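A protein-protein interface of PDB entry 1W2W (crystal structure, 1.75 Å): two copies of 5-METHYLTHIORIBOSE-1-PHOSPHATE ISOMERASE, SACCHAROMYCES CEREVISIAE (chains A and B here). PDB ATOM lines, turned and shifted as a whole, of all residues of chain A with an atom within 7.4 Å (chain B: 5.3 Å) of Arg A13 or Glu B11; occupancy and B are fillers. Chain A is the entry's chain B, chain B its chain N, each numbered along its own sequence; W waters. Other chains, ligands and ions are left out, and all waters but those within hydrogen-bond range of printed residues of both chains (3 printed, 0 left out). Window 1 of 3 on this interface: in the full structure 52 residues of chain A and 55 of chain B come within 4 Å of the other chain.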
ATOM      1  N   LEU A  10       0.930  -3.720 -29.248  1.00  0.00           N
ATOM      2  CA  LEU A  10       1.724  -4.552 -28.359  1.00  0.00           C
ATOM      3  C   LEU A  10       1.925  -3.857 -27.019  1.00  0.00           C
ATOM      4  O   LEU A  10       2.100  -2.634 -26.981  1.00  0.00           O
ATOM      5  CB  LEU A  10       3.082  -4.814 -29.009  1.00  0.00           C
ATOM      6  CG  LEU A  10       3.128  -5.377 -30.429  1.00  0.00           C
ATOM      7  CD1 LEU A  10       4.583  -5.779 -30.705  1.00  0.00           C
ATOM      8  CD2 LEU A  10       2.205  -6.565 -30.572  1.00  0.00           C
ATOM      9  N   GLU A  11       1.918  -4.630 -25.930  1.00  0.00           N
ATOM     10  CA  GLU A  11       2.189  -4.092 -24.588  1.00  0.00           C
ATOM     11  C   GLU A  11       3.428  -3.190 -24.551  1.00  0.00           C
ATOM     12  O   GLU A  11       3.373  -2.094 -23.991  1.00  0.00           O
ATOM     13  CB  GLU A  11       2.335  -5.239 -23.558  1.00  0.00           C
ATOM     14  CG  GLU A  11       2.843  -4.813 -22.180  1.00  0.00           C
ATOM     15  CD  GLU A  11       2.908  -5.969 -21.194  1.00  0.00           C
ATOM     16  OE1 GLU A  11       2.865  -7.143 -21.651  1.00  0.00           O
ATOM     17  OE2 GLU A  11       3.014  -5.695 -19.967  1.00  0.00           O
ATOM     18  N   THR A  12       4.533  -3.661 -25.131  1.00  0.00           N
ATOM     19  CA  THR A  12       5.791  -2.908 -25.207  1.00  0.00           C
ATOM     20  C   THR A  12       6.491  -2.798 -23.855  1.00  0.00           C
ATOM     21  O   THR A  12       6.662  -1.711 -23.288  1.00  0.00           O
ATOM     22  CB  THR A  12       5.614  -1.512 -25.852  1.00  0.00           C
ATOM     23  OG1 THR A  12       4.824  -1.627 -27.040  1.00  0.00           O
ATOM     24  CG2 THR A  12       6.973  -1.006 -26.371  1.00  0.00           C
ATOM     25  N   ARG A  13       6.919  -3.945 -23.344  1.00  0.00           N
ATOM     26  CA  ARG A  13       7.793  -3.973 -22.173  1.00  0.00           C
ATOM     27  C   ARG A  13       9.109  -3.293 -22.518  1.00  0.00           C
ATOM     28  O   ARG A  13       9.423  -3.146 -23.696  1.00  0.00           O
ATOM     29  CB  ARG A  13       8.057  -5.448 -21.799  1.00  0.00           C
ATOM     30  CG  ARG A  13       6.865  -6.183 -21.170  1.00  0.00           C
ATOM     31  CD  ARG A  13       6.668  -5.846 -19.692  1.00  0.00           C
ATOM     32  NE  ARG A  13       7.827  -6.217 -18.880  1.00  0.00           N
ATOM     33  CZ  ARG A  13       8.255  -5.528 -17.833  1.00  0.00           C
ATOM     34  NH1 ARG A  13       7.628  -4.413 -17.477  1.00  0.00           N
ATOM     35  NH2 ARG A  13       9.317  -5.944 -17.149  1.00  0.00           N
ATOM     36  N   PRO A  14       9.903  -2.886 -21.529  1.00  0.00           N
ATOM     37  CA  PRO A  14       9.534  -2.902 -20.107  1.00  0.00           C
ATOM     38  C   PRO A  14       8.794  -1.661 -19.618  1.00  0.00           C
ATOM     39  O   PRO A  14       8.254  -1.699 -18.514  1.00  0.00           O
ATOM     40  CB  PRO A  14      10.896  -2.965 -19.400  1.00  0.00           C
ATOM     41  CG  PRO A  14      11.826  -2.257 -20.328  1.00  0.00           C
ATOM     42  CD  PRO A  14      11.284  -2.415 -21.742  1.00  0.00           C
ATOM     43  N   TYR A  15       8.782  -0.580 -20.396  1.00  0.00           N
ATOM     44  CA  TYR A  15       8.198   0.670 -19.922  1.00  0.00           C
ATOM     45  C   TYR A  15       6.671   0.613 -20.028  1.00  0.00           C
ATOM     46  O   TYR A  15       5.969   1.331 -19.318  1.00  0.00           O
ATOM     47  CB  TYR A  15       8.767   1.834 -20.742  1.00  0.00           C
ATOM     48  CG  TYR A  15       8.275   3.231 -20.419  1.00  0.00           C
ATOM     49  CD1 TYR A  15       9.029   4.090 -19.622  1.00  0.00           C
ATOM     50  CD2 TYR A  15       7.070   3.709 -20.937  1.00  0.00           C
ATOM     51  CE1 TYR A  15       8.575   5.384 -19.330  1.00  0.00           C
ATOM     52  CE2 TYR A  15       6.628   4.999 -20.662  1.00  0.00           C
ATOM     53  CZ  TYR A  15       7.375   5.828 -19.858  1.00  0.00           C
ATOM     54  OH  TYR A  15       6.906   7.103 -19.595  1.00  0.00           O
ATOM     55  N   ASN A  16       6.181  -0.264 -20.903  1.00  0.00           N
ATOM     56  CA  ASN A  16       4.755  -0.429 -21.163  1.00  0.00           C
ATOM     57  C   ASN A  16       4.102   0.750 -21.870  1.00  0.00           C
ATOM     58  O   ASN A  16       2.982   1.124 -21.520  1.00  0.00           O
ATOM     59  CB  ASN A  16       4.007  -0.802 -19.882  1.00  0.00           C
ATOM     60  CG  ASN A  16       4.432  -2.154 -19.353  1.00  0.00           C
ATOM     61  OD1 ASN A  16       4.930  -2.971 -20.112  1.00  0.00           O
ATOM     62  ND2 ASN A  16       4.280  -2.382 -18.045  1.00  0.00           N
ATOM     63  N   GLN A  17       4.798   1.327 -22.859  1.00  0.00           N
ATOM     64  CA  GLN A  17       4.198   2.360 -23.716  1.00  0.00           C
ATOM     65  C   GLN A  17       2.903   1.900 -24.370  1.00  0.00           C
ATOM     66  O   GLN A  17       1.984   2.690 -24.603  1.00  0.00           O
ATOM     67  CB  GLN A  17       5.151   2.744 -24.851  1.00  0.00           C
ATOM     68  CG  GLN A  17       6.320   3.626 -24.419  1.00  0.00           C
ATOM     69  CD  GLN A  17       7.536   2.818 -24.016  1.00  0.00           C
ATOM     70  OE1 GLN A  17       7.419   1.618 -23.731  1.00  0.00           O
ATOM     71  NE2 GLN A  17       8.710   3.466 -23.995  1.00  0.00           N
ATOM     72  N   GLY A  18       2.846   0.620 -24.705  1.00  0.00           N
ATOM     73  CA  GLY A  18       1.691   0.089 -25.410  1.00  0.00           C
ATOM     74  C   GLY A  18       0.490  -0.021 -24.496  1.00  0.00           C
ATOM     75  O   GLY A  18      -0.616   0.457 -24.812  1.00  0.00           O
ATOM     76  N   SER A  19       0.686  -0.670 -23.350  1.00  0.00           N
ATOM     77  CA  SER A  19      -0.449  -0.997 -22.503  1.00  0.00           C
ATOM     78  C   SER A  19      -0.924   0.238 -21.729  1.00  0.00           C
ATOM     79  O   SER A  19      -2.123   0.415 -21.469  1.00  0.00           O
ATOM     80  CB  SER A  19      -0.098  -2.160 -21.562  1.00  0.00           C
ATOM     81  OG  SER A  19       0.832  -1.755 -20.567  1.00  0.00           O
ATOM     82  N   THR A  37       0.204  -9.291 -25.740  1.00  0.00           N
ATOM     83  CA  THR A  37       1.574  -9.289 -25.224  1.00  0.00           C
ATOM     84  C   THR A  37       2.555  -9.172 -26.387  1.00  0.00           C
ATOM     85  O   THR A  37       2.244  -9.503 -27.528  1.00  0.00           O
ATOM     86  CB  THR A  37       1.913 -10.575 -24.434  1.00  0.00           C
ATOM     87  OG1 THR A  37       1.986 -11.689 -25.341  1.00  0.00           O
ATOM     88  CG2 THR A  37       0.808 -10.945 -23.427  1.00  0.00           C
ATOM     89  N   ASP A  38       3.766  -8.711 -26.094  1.00  0.00           N
ATOM     90  CA  ASP A  38       4.797  -8.685 -27.118  1.00  0.00           C
ATOM     91  C   ASP A  38       5.032 -10.079 -27.692  1.00  0.00           C
ATOM     92  O   ASP A  38       5.354 -10.244 -28.878  1.00  0.00           O
ATOM     93  CB  ASP A  38       6.096  -8.136 -26.526  1.00  0.00           C
ATOM     94  CG  ASP A  38       5.925  -6.743 -25.958  1.00  0.00           C
ATOM     95  OD1 ASP A  38       5.171  -5.940 -26.572  1.00  0.00           O
ATOM     96  OD2 ASP A  38       6.511  -6.374 -24.916  1.00  0.00           O
ATOM     97  N   LYS A  71      11.806   1.614 -30.628  1.00  0.00           N
ATOM     98  CA  LYS A  71      11.612   0.891 -29.372  1.00  0.00           C
ATOM     99  C   LYS A  71      12.069  -0.572 -29.497  1.00  0.00           C
ATOM    100  O   LYS A  71      11.769  -1.234 -30.489  1.00  0.00           O
ATOM    101  CB  LYS A  71      10.128   0.957 -28.975  1.00  0.00           C
ATOM    102  CG  LYS A  71       9.816   0.364 -27.577  1.00  0.00           C
ATOM    103  CD  LYS A  71      10.753   0.910 -26.497  1.00  0.00           C
ATOM    104  CE  LYS A  71      10.817   2.445 -26.553  1.00  0.00           C
ATOM    105  NZ  LYS A  71      11.894   2.896 -25.605  1.00  0.00           N
ATOM    106  N   ILE A  72      12.786  -1.062 -28.485  1.00  0.00           N
ATOM    107  CA  ILE A  72      13.099  -2.487 -28.353  1.00  0.00           C
ATOM    108  C   ILE A  72      11.866  -3.352 -28.679  1.00  0.00           C
ATOM    109  O   ILE A  72      10.776  -3.138 -28.148  1.00  0.00           O
ATOM    110  CB  ILE A  72      13.652  -2.764 -26.929  1.00  0.00           C
ATOM    111  CG1 ILE A  72      14.155  -4.206 -26.790  1.00  0.00           C
ATOM    112  CG2 ILE A  72      12.621  -2.424 -25.856  1.00  0.00           C
ATOM    113  CD1 ILE A  72      15.270  -4.565 -27.803  1.00  0.00           C
ATOM    114  N   GLY A  73      12.041  -4.313 -29.581  1.00  0.00           N
ATOM    115  CA  GLY A  73      10.920  -5.102 -30.074  1.00  0.00           C
ATOM    116  C   GLY A  73      10.580  -4.801 -31.519  1.00  0.00           C
ATOM    117  O   GLY A  73       9.893  -5.579 -32.179  1.00  0.00           O
ATOM    118  N   GLU A 116      14.349  -0.621 -13.973  1.00  0.00           N
ATOM    119  CA  GLU A 116      13.205  -0.223 -14.793  1.00  0.00           C
ATOM    120  C   GLU A 116      12.609  -1.415 -15.536  1.00  0.00           C
ATOM    121  O   GLU A 116      11.520  -1.317 -16.088  1.00  0.00           O
ATOM    122  CB  GLU A 116      13.599   0.870 -15.799  1.00  0.00           C
ATOM    123  CG  GLU A 116      13.973   2.191 -15.137  1.00  0.00           C
ATOM    124  CD  GLU A 116      14.381   3.255 -16.137  1.00  0.00           C
ATOM    125  OE1 GLU A 116      14.123   3.079 -17.347  1.00  0.00           O
ATOM    126  OE2 GLU A 116      14.963   4.275 -15.709  1.00  0.00           O
ATOM    127  N   PHE A 117      13.341  -2.528 -15.555  1.00  0.00           N
ATOM    128  CA  PHE A 117      12.920  -3.796 -16.178  1.00  0.00           C
ATOM    129  C   PHE A 117      12.340  -4.663 -15.053  1.00  0.00           C
ATOM    130  O   PHE A 117      11.229  -5.180 -15.159  1.00  0.00           O
ATOM    131  CB  PHE A 117      14.178  -4.433 -16.811  1.00  0.00           C
ATOM    132  CG  PHE A 117      14.005  -5.828 -17.402  1.00  0.00           C
ATOM    133  CD1 PHE A 117      14.601  -6.131 -18.615  1.00  0.00           C
ATOM    134  CD2 PHE A 117      13.326  -6.833 -16.746  1.00  0.00           C
ATOM    135  CE1 PHE A 117      14.493  -7.387 -19.183  1.00  0.00           C
ATOM    136  CE2 PHE A 117      13.209  -8.105 -17.313  1.00  0.00           C
ATOM    137  CZ  PHE A 117      13.796  -8.378 -18.536  1.00  0.00           C
ATOM    138  N   LYS A 118      13.081  -4.807 -13.953  1.00  0.00           N
ATOM    139  CA  LYS A 118      12.698  -5.734 -12.892  1.00  0.00           C
ATOM    140  C   LYS A 118      11.566  -5.221 -12.011  1.00  0.00           C
ATOM    141  O   LYS A 118      10.943  -6.002 -11.291  1.00  0.00           O
ATOM    142  CB  LYS A 118      13.914  -6.089 -12.019  1.00  0.00           C
ATOM    143  CG  LYS A 118      15.095  -6.562 -12.854  1.00  0.00           C
ATOM    144  CD  LYS A 118      15.989  -7.554 -12.102  1.00  0.00           C
ATOM    145  CE  LYS A 118      17.218  -6.903 -11.535  1.00  0.00           C
ATOM    146  NZ  LYS A 118      17.906  -7.843 -10.592  1.00  0.00           N
ATOM    147  N   VAL A 119      11.311  -3.919 -12.044  1.00  0.00           N
ATOM    148  CA  VAL A 119      10.215  -3.363 -11.250  1.00  0.00           C
ATOM    149  C   VAL A 119       9.192  -2.750 -12.185  1.00  0.00           C
ATOM    150  O   VAL A 119       9.554  -1.974 -13.069  1.00  0.00           O
ATOM    151  CB  VAL A 119      10.725  -2.306 -10.253  1.00  0.00           C
ATOM    152  CG1 VAL A 119       9.566  -1.689  -9.462  1.00  0.00           C
ATOM    153  CG2 VAL A 119      11.713  -2.944  -9.300  1.00  0.00           C
ATOM    154  N   VAL A 120       7.925  -3.118 -11.989  1.00  0.00           N
ATOM    155  CA  VAL A 120       6.829  -2.632 -12.813  1.00  0.00           C
ATOM    156  C   VAL A 120       6.059  -1.533 -12.077  1.00  0.00           C
ATOM    157  O   VAL A 120       5.679  -1.698 -10.910  1.00  0.00           O
ATOM    158  CB  VAL A 120       5.871  -3.793 -13.160  1.00  0.00           C
ATOM    159  CG1 VAL A 120       4.678  -3.305 -13.999  1.00  0.00           C
ATOM    160  CG2 VAL A 120       6.632  -4.891 -13.922  1.00  0.00           C
ATOM    161  N   THR A 121       5.832  -0.418 -12.766  1.00  0.00           N
ATOM    162  CA  THR A 121       5.068   0.699 -12.214  1.00  0.00           C
ATOM    163  C   THR A 121       3.634   0.617 -12.732  1.00  0.00           C
ATOM    164  O   THR A 121       3.404   0.311 -13.903  1.00  0.00           O
ATOM    165  CB  THR A 121       5.707   2.014 -12.687  1.00  0.00           C
ATOM    166  OG1 THR A 121       7.034   2.115 -12.152  1.00  0.00           O
ATOM    167  CG2 THR A 121       4.972   3.223 -12.107  1.00  0.00           C
ATOM    168  N   ILE A 147       9.324  -8.040 -10.053  1.00  0.00           N
ATOM    169  CA  ILE A 147       8.943  -9.292 -10.716  1.00  0.00           C
ATOM    170  C   ILE A 147      10.149 -10.191 -11.037  1.00  0.00           C
ATOM    171  O   ILE A 147      10.058 -11.108 -11.856  1.00  0.00           O
ATOM    172  CB  ILE A 147       8.099  -9.006 -11.986  1.00  0.00           C
ATOM    173  CG1 ILE A 147       8.844  -8.080 -12.952  1.00  0.00           C
ATOM    174  CG2 ILE A 147       6.768  -8.350 -11.578  1.00  0.00           C
ATOM    175  CD1 ILE A 147       8.485  -8.279 -14.413  1.00  0.00           C
ATOM    176  N   ASN A 156      18.722  -4.436 -20.702  1.00  0.00           N
ATOM    177  CA  ASN A 156      17.658  -3.434 -20.841  1.00  0.00           C
ATOM    178  C   ASN A 156      17.951  -2.358 -21.881  1.00  0.00           C
ATOM    179  O   ASN A 156      18.002  -1.173 -21.545  1.00  0.00           O
ATOM    180  CB  ASN A 156      17.365  -2.794 -19.482  1.00  0.00           C
ATOM    181  CG  ASN A 156      16.020  -2.090 -19.446  1.00  0.00           C
ATOM    182  OD1 ASN A 156      15.146  -2.382 -20.257  1.00  0.00           O
ATOM    183  ND2 ASN A 156      15.852  -1.161 -18.510  1.00  0.00           N
ATOM    184  N   PRO A 157      18.141  -2.748 -23.143  1.00  0.00           N
ATOM    185  CA  PRO A 157      18.274  -1.760 -24.224  1.00  0.00           C
ATOM    186  C   PRO A 157      16.925  -1.102 -24.462  1.00  0.00           C
ATOM    187  O   PRO A 157      15.926  -1.818 -24.496  1.00  0.00           O
ATOM    188  CB  PRO A 157      18.639  -2.619 -25.433  1.00  0.00           C
ATOM    189  CG  PRO A 157      17.999  -3.951 -25.151  1.00  0.00           C
ATOM    190  CD  PRO A 157      18.237  -4.129 -23.650  1.00  0.00           C
ATOM    191  N   ALA A 158      16.893   0.222 -24.606  1.00  0.00           N
ATOM    192  CA  ALA A 158      15.631   0.928 -24.827  1.00  0.00           C
ATOM    193  C   ALA A 158      15.200   0.850 -26.293  1.00  0.00           C
ATOM    194  O   ALA A 158      14.043   1.152 -26.636  1.00  0.00           O
ATOM    195  CB  ALA A 158      15.767   2.386 -24.396  1.00  0.00           C
ATOM    196  N   PRO B   9      16.981 -16.482 -20.523  1.00  0.00           N
ATOM    197  CA  PRO B   9      15.548 -16.758 -20.335  1.00  0.00           C
ATOM    198  C   PRO B   9      14.684 -15.546 -20.694  1.00  0.00           C
ATOM    199  O   PRO B   9      15.102 -14.419 -20.448  1.00  0.00           O
ATOM    200  CB  PRO B   9      15.452 -17.066 -18.833  1.00  0.00           C
ATOM    201  CG  PRO B   9      16.569 -16.236 -18.217  1.00  0.00           C
ATOM    202  CD  PRO B   9      17.679 -16.222 -19.253  1.00  0.00           C
ATOM    203  N   LEU B  10      13.506 -15.779 -21.269  1.00  0.00           N
ATOM    204  CA  LEU B  10      12.538 -14.711 -21.508  1.00  0.00           C
ATOM    205  C   LEU B  10      11.646 -14.496 -20.293  1.00  0.00           C
ATOM    206  O   LEU B  10      11.254 -15.450 -19.605  1.00  0.00           O
ATOM    207  CB  LEU B  10      11.634 -15.073 -22.687  1.00  0.00           C
ATOM    208  CG  LEU B  10      12.356 -15.583 -23.935  1.00  0.00           C
ATOM    209  CD1 LEU B  10      11.343 -15.749 -25.054  1.00  0.00           C
ATOM    210  CD2 LEU B  10      13.472 -14.631 -24.356  1.00  0.00           C
ATOM    211  N   GLU B  11      11.303 -13.233 -20.063  1.00  0.00           N
ATOM    212  CA  GLU B  11      10.410 -12.846 -18.977  1.00  0.00           C
ATOM    213  C   GLU B  11       9.142 -13.704 -18.993  1.00  0.00           C
ATOM    214  O   GLU B  11       8.674 -14.124 -17.944  1.00  0.00           O
ATOM    215  CB  GLU B  11      10.026 -11.368 -19.145  1.00  0.00           C
ATOM    216  CG  GLU B  11       8.955 -10.878 -18.183  1.00  0.00           C
ATOM    217  CD  GLU B  11       8.631  -9.395 -18.347  1.00  0.00           C
ATOM    218  OE1 GLU B  11       9.102  -8.757 -19.332  1.00  0.00           O
ATOM    219  OE2 GLU B  11       7.892  -8.875 -17.473  1.00  0.00           O
ATOM    220  N   THR B  12       8.602 -13.940 -20.184  1.00  0.00           N
ATOM    221  CA  THR B  12       7.367 -14.714 -20.370  1.00  0.00           C
ATOM    222  C   THR B  12       6.132 -14.077 -19.732  1.00  0.00           C
ATOM    223  O   THR B  12       5.561 -14.613 -18.775  1.00  0.00           O
ATOM    224  CB  THR B  12       7.527 -16.186 -19.907  1.00  0.00           C
ATOM    225  OG1 THR B  12       8.789 -16.691 -20.349  1.00  0.00           O
ATOM    226  CG2 THR B  12       6.515 -17.089 -20.640  1.00  0.00           C
ATOM    227  N   ARG B  13       5.723 -12.940 -20.290  1.00  0.00           N
ATOM    228  CA  ARG B  13       4.429 -12.336 -19.977  1.00  0.00           C
ATOM    229  C   ARG B  13       3.288 -13.306 -20.320  1.00  0.00           C
ATOM    230  O   ARG B  13       3.478 -14.228 -21.104  1.00  0.00           O
ATOM    231  CB  ARG B  13       4.265 -11.036 -20.782  1.00  0.00           C
ATOM    232  CG  ARG B  13       5.114  -9.847 -20.290  1.00  0.00           C
ATOM    233  CD  ARG B  13       4.555  -9.193 -19.035  1.00  0.00           C
ATOM    234  NE  ARG B  13       3.250  -8.583 -19.292  1.00  0.00           N
ATOM    235  CZ  ARG B  13       2.265  -8.526 -18.401  1.00  0.00           C
ATOM    236  NH1 ARG B  13       2.419  -9.053 -17.192  1.00  0.00           N
ATOM    237  NH2 ARG B  13       1.120  -7.946 -18.733  1.00  0.00           N
ATOM    238  N   ASN B  16       4.562 -14.178 -16.076  1.00  0.00           N
ATOM    239  CA  ASN B  16       5.970 -13.986 -15.728  1.00  0.00           C
ATOM    240  C   ASN B  16       6.700 -15.215 -15.174  1.00  0.00           C
ATOM    241  O   ASN B  16       7.520 -15.108 -14.253  1.00  0.00           O
ATOM    242  CB  ASN B  16       6.159 -12.762 -14.832  1.00  0.00           C
ATOM    243  CG  ASN B  16       5.772 -11.478 -15.533  1.00  0.00           C
ATOM    244  OD1 ASN B  16       5.803 -11.409 -16.761  1.00  0.00           O
ATOM    245  ND2 ASN B  16       5.394 -10.460 -14.764  1.00  0.00           N
ATOM    246  N   GLN B  17       6.413 -16.383 -15.744  1.00  0.00           N
ATOM    247  CA  GLN B  17       7.169 -17.590 -15.389  1.00  0.00           C
ATOM    248  C   GLN B  17       8.679 -17.432 -15.530  1.00  0.00           C
ATOM    249  O   GLN B  17       9.432 -18.066 -14.784  1.00  0.00           O
ATOM    250  CB  GLN B  17       6.761 -18.790 -16.266  1.00  0.00           C
ATOM    251  CG  GLN B  17       5.381 -19.348 -15.989  1.00  0.00           C
ATOM    252  CD  GLN B  17       4.297 -18.689 -16.823  1.00  0.00           C
ATOM    253  OE1 GLN B  17       4.487 -17.587 -17.354  1.00  0.00           O
ATOM    254  NE2 GLN B  17       3.152 -19.355 -16.929  1.00  0.00           N
ATOM    255  N   GLY B  18       9.117 -16.625 -16.495  1.00  0.00           N
ATOM    256  CA  GLY B  18      10.532 -16.489 -16.799  1.00  0.00           C
ATOM    257  C   GLY B  18      11.224 -15.628 -15.761  1.00  0.00           C
ATOM    258  O   GLY B  18      12.249 -15.993 -15.195  1.00  0.00           O
ATOM    259  N   SER B  19      10.659 -14.456 -15.493  1.00  0.00           N
ATOM    260  CA  SER B  19      11.302 -13.542 -14.563  1.00  0.00           C
ATOM    261  C   SER B  19      11.156 -13.951 -13.097  1.00  0.00           C
ATOM    262  O   SER B  19      12.099 -13.789 -12.324  1.00  0.00           O
ATOM    263  CB  SER B  19      10.820 -12.110 -14.817  1.00  0.00           C
ATOM    264  OG  SER B  19       9.495 -11.926 -14.353  1.00  0.00           O
ATOM    265  N   LEU B  35      18.369 -12.257 -18.003  1.00  0.00           N
ATOM    266  CA  LEU B  35      16.953 -12.241 -18.336  1.00  0.00           C
ATOM    267  C   LEU B  35      16.681 -11.137 -19.360  1.00  0.00           C
ATOM    268  O   LEU B  35      17.226 -10.030 -19.249  1.00  0.00           O
ATOM    269  CB  LEU B  35      16.174 -11.989 -17.046  1.00  0.00           C
ATOM    270  CG  LEU B  35      14.672 -11.729 -17.121  1.00  0.00           C
ATOM    271  CD1 LEU B  35      13.929 -13.027 -17.490  1.00  0.00           C
ATOM    272  CD2 LEU B  35      14.245 -11.175 -15.770  1.00  0.00           C
ATOM    273  N   ILE B  36      15.857 -11.438 -20.361  1.00  0.00           N
ATOM    274  CA  ILE B  36      15.554 -10.451 -21.393  1.00  0.00           C
ATOM    275  C   ILE B  36      14.044 -10.335 -21.563  1.00  0.00           C
ATOM    276  O   ILE B  36      13.309 -11.256 -21.199  1.00  0.00           O
ATOM    277  CB  ILE B  36      16.242 -10.797 -22.741  1.00  0.00           C
ATOM    278  CG1 ILE B  36      15.648 -12.072 -23.353  1.00  0.00           C
ATOM    279  CG2 ILE B  36      17.763 -10.937 -22.566  1.00  0.00           C
ATOM    280  CD1 ILE B  36      16.245 -12.434 -24.738  1.00  0.00           C
ATOM    281  N   THR B  37      13.573  -9.211 -22.097  1.00  0.00           N
ATOM    282  CA  THR B  37      12.151  -9.137 -22.428  1.00  0.00           C
ATOM    283  C   THR B  37      11.795 -10.121 -23.537  1.00  0.00           C
ATOM    284  O   THR B  37      12.646 -10.532 -24.335  1.00  0.00           O
ATOM    285  CB  THR B  37      11.690  -7.709 -22.846  1.00  0.00           C
ATOM    286  OG1 THR B  37      12.212  -7.380 -24.148  1.00  0.00           O
ATOM    287  CG2 THR B  37      12.237  -6.603 -21.900  1.00  0.00           C
ATOM    288  N   ASP B  38      10.521 -10.491 -23.602  1.00  0.00           N
ATOM    289  CA  ASP B  38      10.051 -11.337 -24.696  1.00  0.00           C
ATOM    290  C   ASP B  38      10.346 -10.680 -26.038  1.00  0.00           C
ATOM    291  O   ASP B  38      10.649 -11.360 -27.014  1.00  0.00           O
ATOM    292  CB  ASP B  38       8.554 -11.645 -24.567  1.00  0.00           C
ATOM    293  CG  ASP B  38       8.199 -12.286 -23.240  1.00  0.00           C
ATOM    294  OD1 ASP B  38       8.971 -13.136 -22.738  1.00  0.00           O
ATOM    295  OD2 ASP B  38       7.152 -11.988 -22.620  1.00  0.00           O
ATOM    296  N   SER B  39      10.281  -9.352 -26.079  1.00  0.00           N
ATOM    297  CA  SER B  39      10.445  -8.608 -27.322  1.00  0.00           C
ATOM    298  C   SER B  39      11.895  -8.477 -27.790  1.00  0.00           C
ATOM    299  O   SER B  39      12.155  -7.955 -28.878  1.00  0.00           O
ATOM    300  CB  SER B  39       9.843  -7.210 -27.156  1.00  0.00           C
ATOM    301  OG  SER B  39      10.590  -6.467 -26.202  1.00  0.00           O
HETATM  302  O   HOH W   1       9.173  -4.180 -26.207  1.00  0.00           O
HETATM  303  O   HOH W   2       5.302 -10.583 -24.033  1.00  0.00           O
HETATM  304  O   HOH W   3       8.578  -8.013 -24.157  1.00  0.00           O
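The side-chain carboxylate of Glu A11 lies within salt-bridge range of the guanidinium group of Arg B13 (2.8 Å). OE1 of Glu B11 is in salt-bridge range of NE of Arg A13 (2.9 Å). The backbone carbonyl oxygen of Ile A147 sits at hydrogen-bond distance from the side-chain hydroxyl of Ser B19, 2.7 Å away.
The side-chain amide oxygen of Asn A16 sits close to the side-chain carboxylate of Glu A11. OD2 of Asp A38 is in hydrogen-bond range of N of Arg A13, 2.9 Å away. N of Ile A72 sits at hydrogen-bond distance from O of Ala A158 (3.1 Å). The backbone carbonyl oxygen (O) of Lys A118 lies within hydrogen-bond range of the backbone NH (N) of Ile A147 (2.9 Å). O of Pro B9 is in hydrogen-bond range of N of Ile B36 (3.1 Å). N of Gly B18 is in hydrogen-bond range of O of Glu B11.
Asp A38 touches Ser B39. Ile A72 touches Ser B39 (O to OG, 3.9 Å). CA of Gly A73 touches O of Ser B39, at 3.3 Å. Leu B35 touches Phe A117. CZ of Phe A117 touches C of Ile B36, at 3.6 Å. Phe A117 touches Thr B37 (CE1 to N, 3.6 Å). Glu B11 touches Ile A147 (OE2 to CD1, 3.2 Å). Ile A147 touches Asn B16.
Of the printed residues of chain B, Arg A13 touches Glu B11 (2.9 Å). Glu B11 touches two residues of chain A. Of the printed residues of chain A, Asn B16 touches Ile A147 (3.8 Å). Printed residues of chain B within 4 Å of Glu A11: Arg B13. Printed residues of chain A within 4 Å of Ser B19: Ile A147. Of the printed residues of chain B, Phe A117 touches Leu B35, Ile B36 and Thr B37. Printed residues of chain A within 4 Å of Leu B35: Phe A117 (3.6 Å). Gln A17 touches none of the printed residues of chain B.
Hydrophobic or aromatic side chains of chain B within 4 Å of the printed part of chain A: Leu B35. Along chain B the printed residues that touch a printed residue of chain A span positions 11 to 39. Of the 25 printed residues of chain A, 7 touch a printed residue of chain B. Along chain A the printed residues that touch a printed residue of chain B span positions 11 to 147.
Glu A11 touches Arg B13, and with the chains exchanged Arg A13 touches Glu B11. Positions printed for both chains: 10, 11, 12, 13, 16, 17, 18, 19, 37 and 38. Of the 11 pairs that touch across the chains among the printed residues, 2 have their exchanged pair printed and touching as well.
Water W1 lies within hydrogen-bond range of OG of Ser B39 (2.7 Å), O of Ile A72 (2.7 Å) and O of Arg A13 (2.7 Å). Water W2 bridges the side-chain carboxylate (OD2) of Asp B38 and the backbone NH (N) of Asp A38. Water W3 lies within hydrogen-bond range of the side-chain carboxylate (OD2) of Asp A38 (2.7 Å), the backbone NH (N) of Ser B39 (2.9 Å) and the backbone NH (N) of Asp B38 (3.2 Å).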
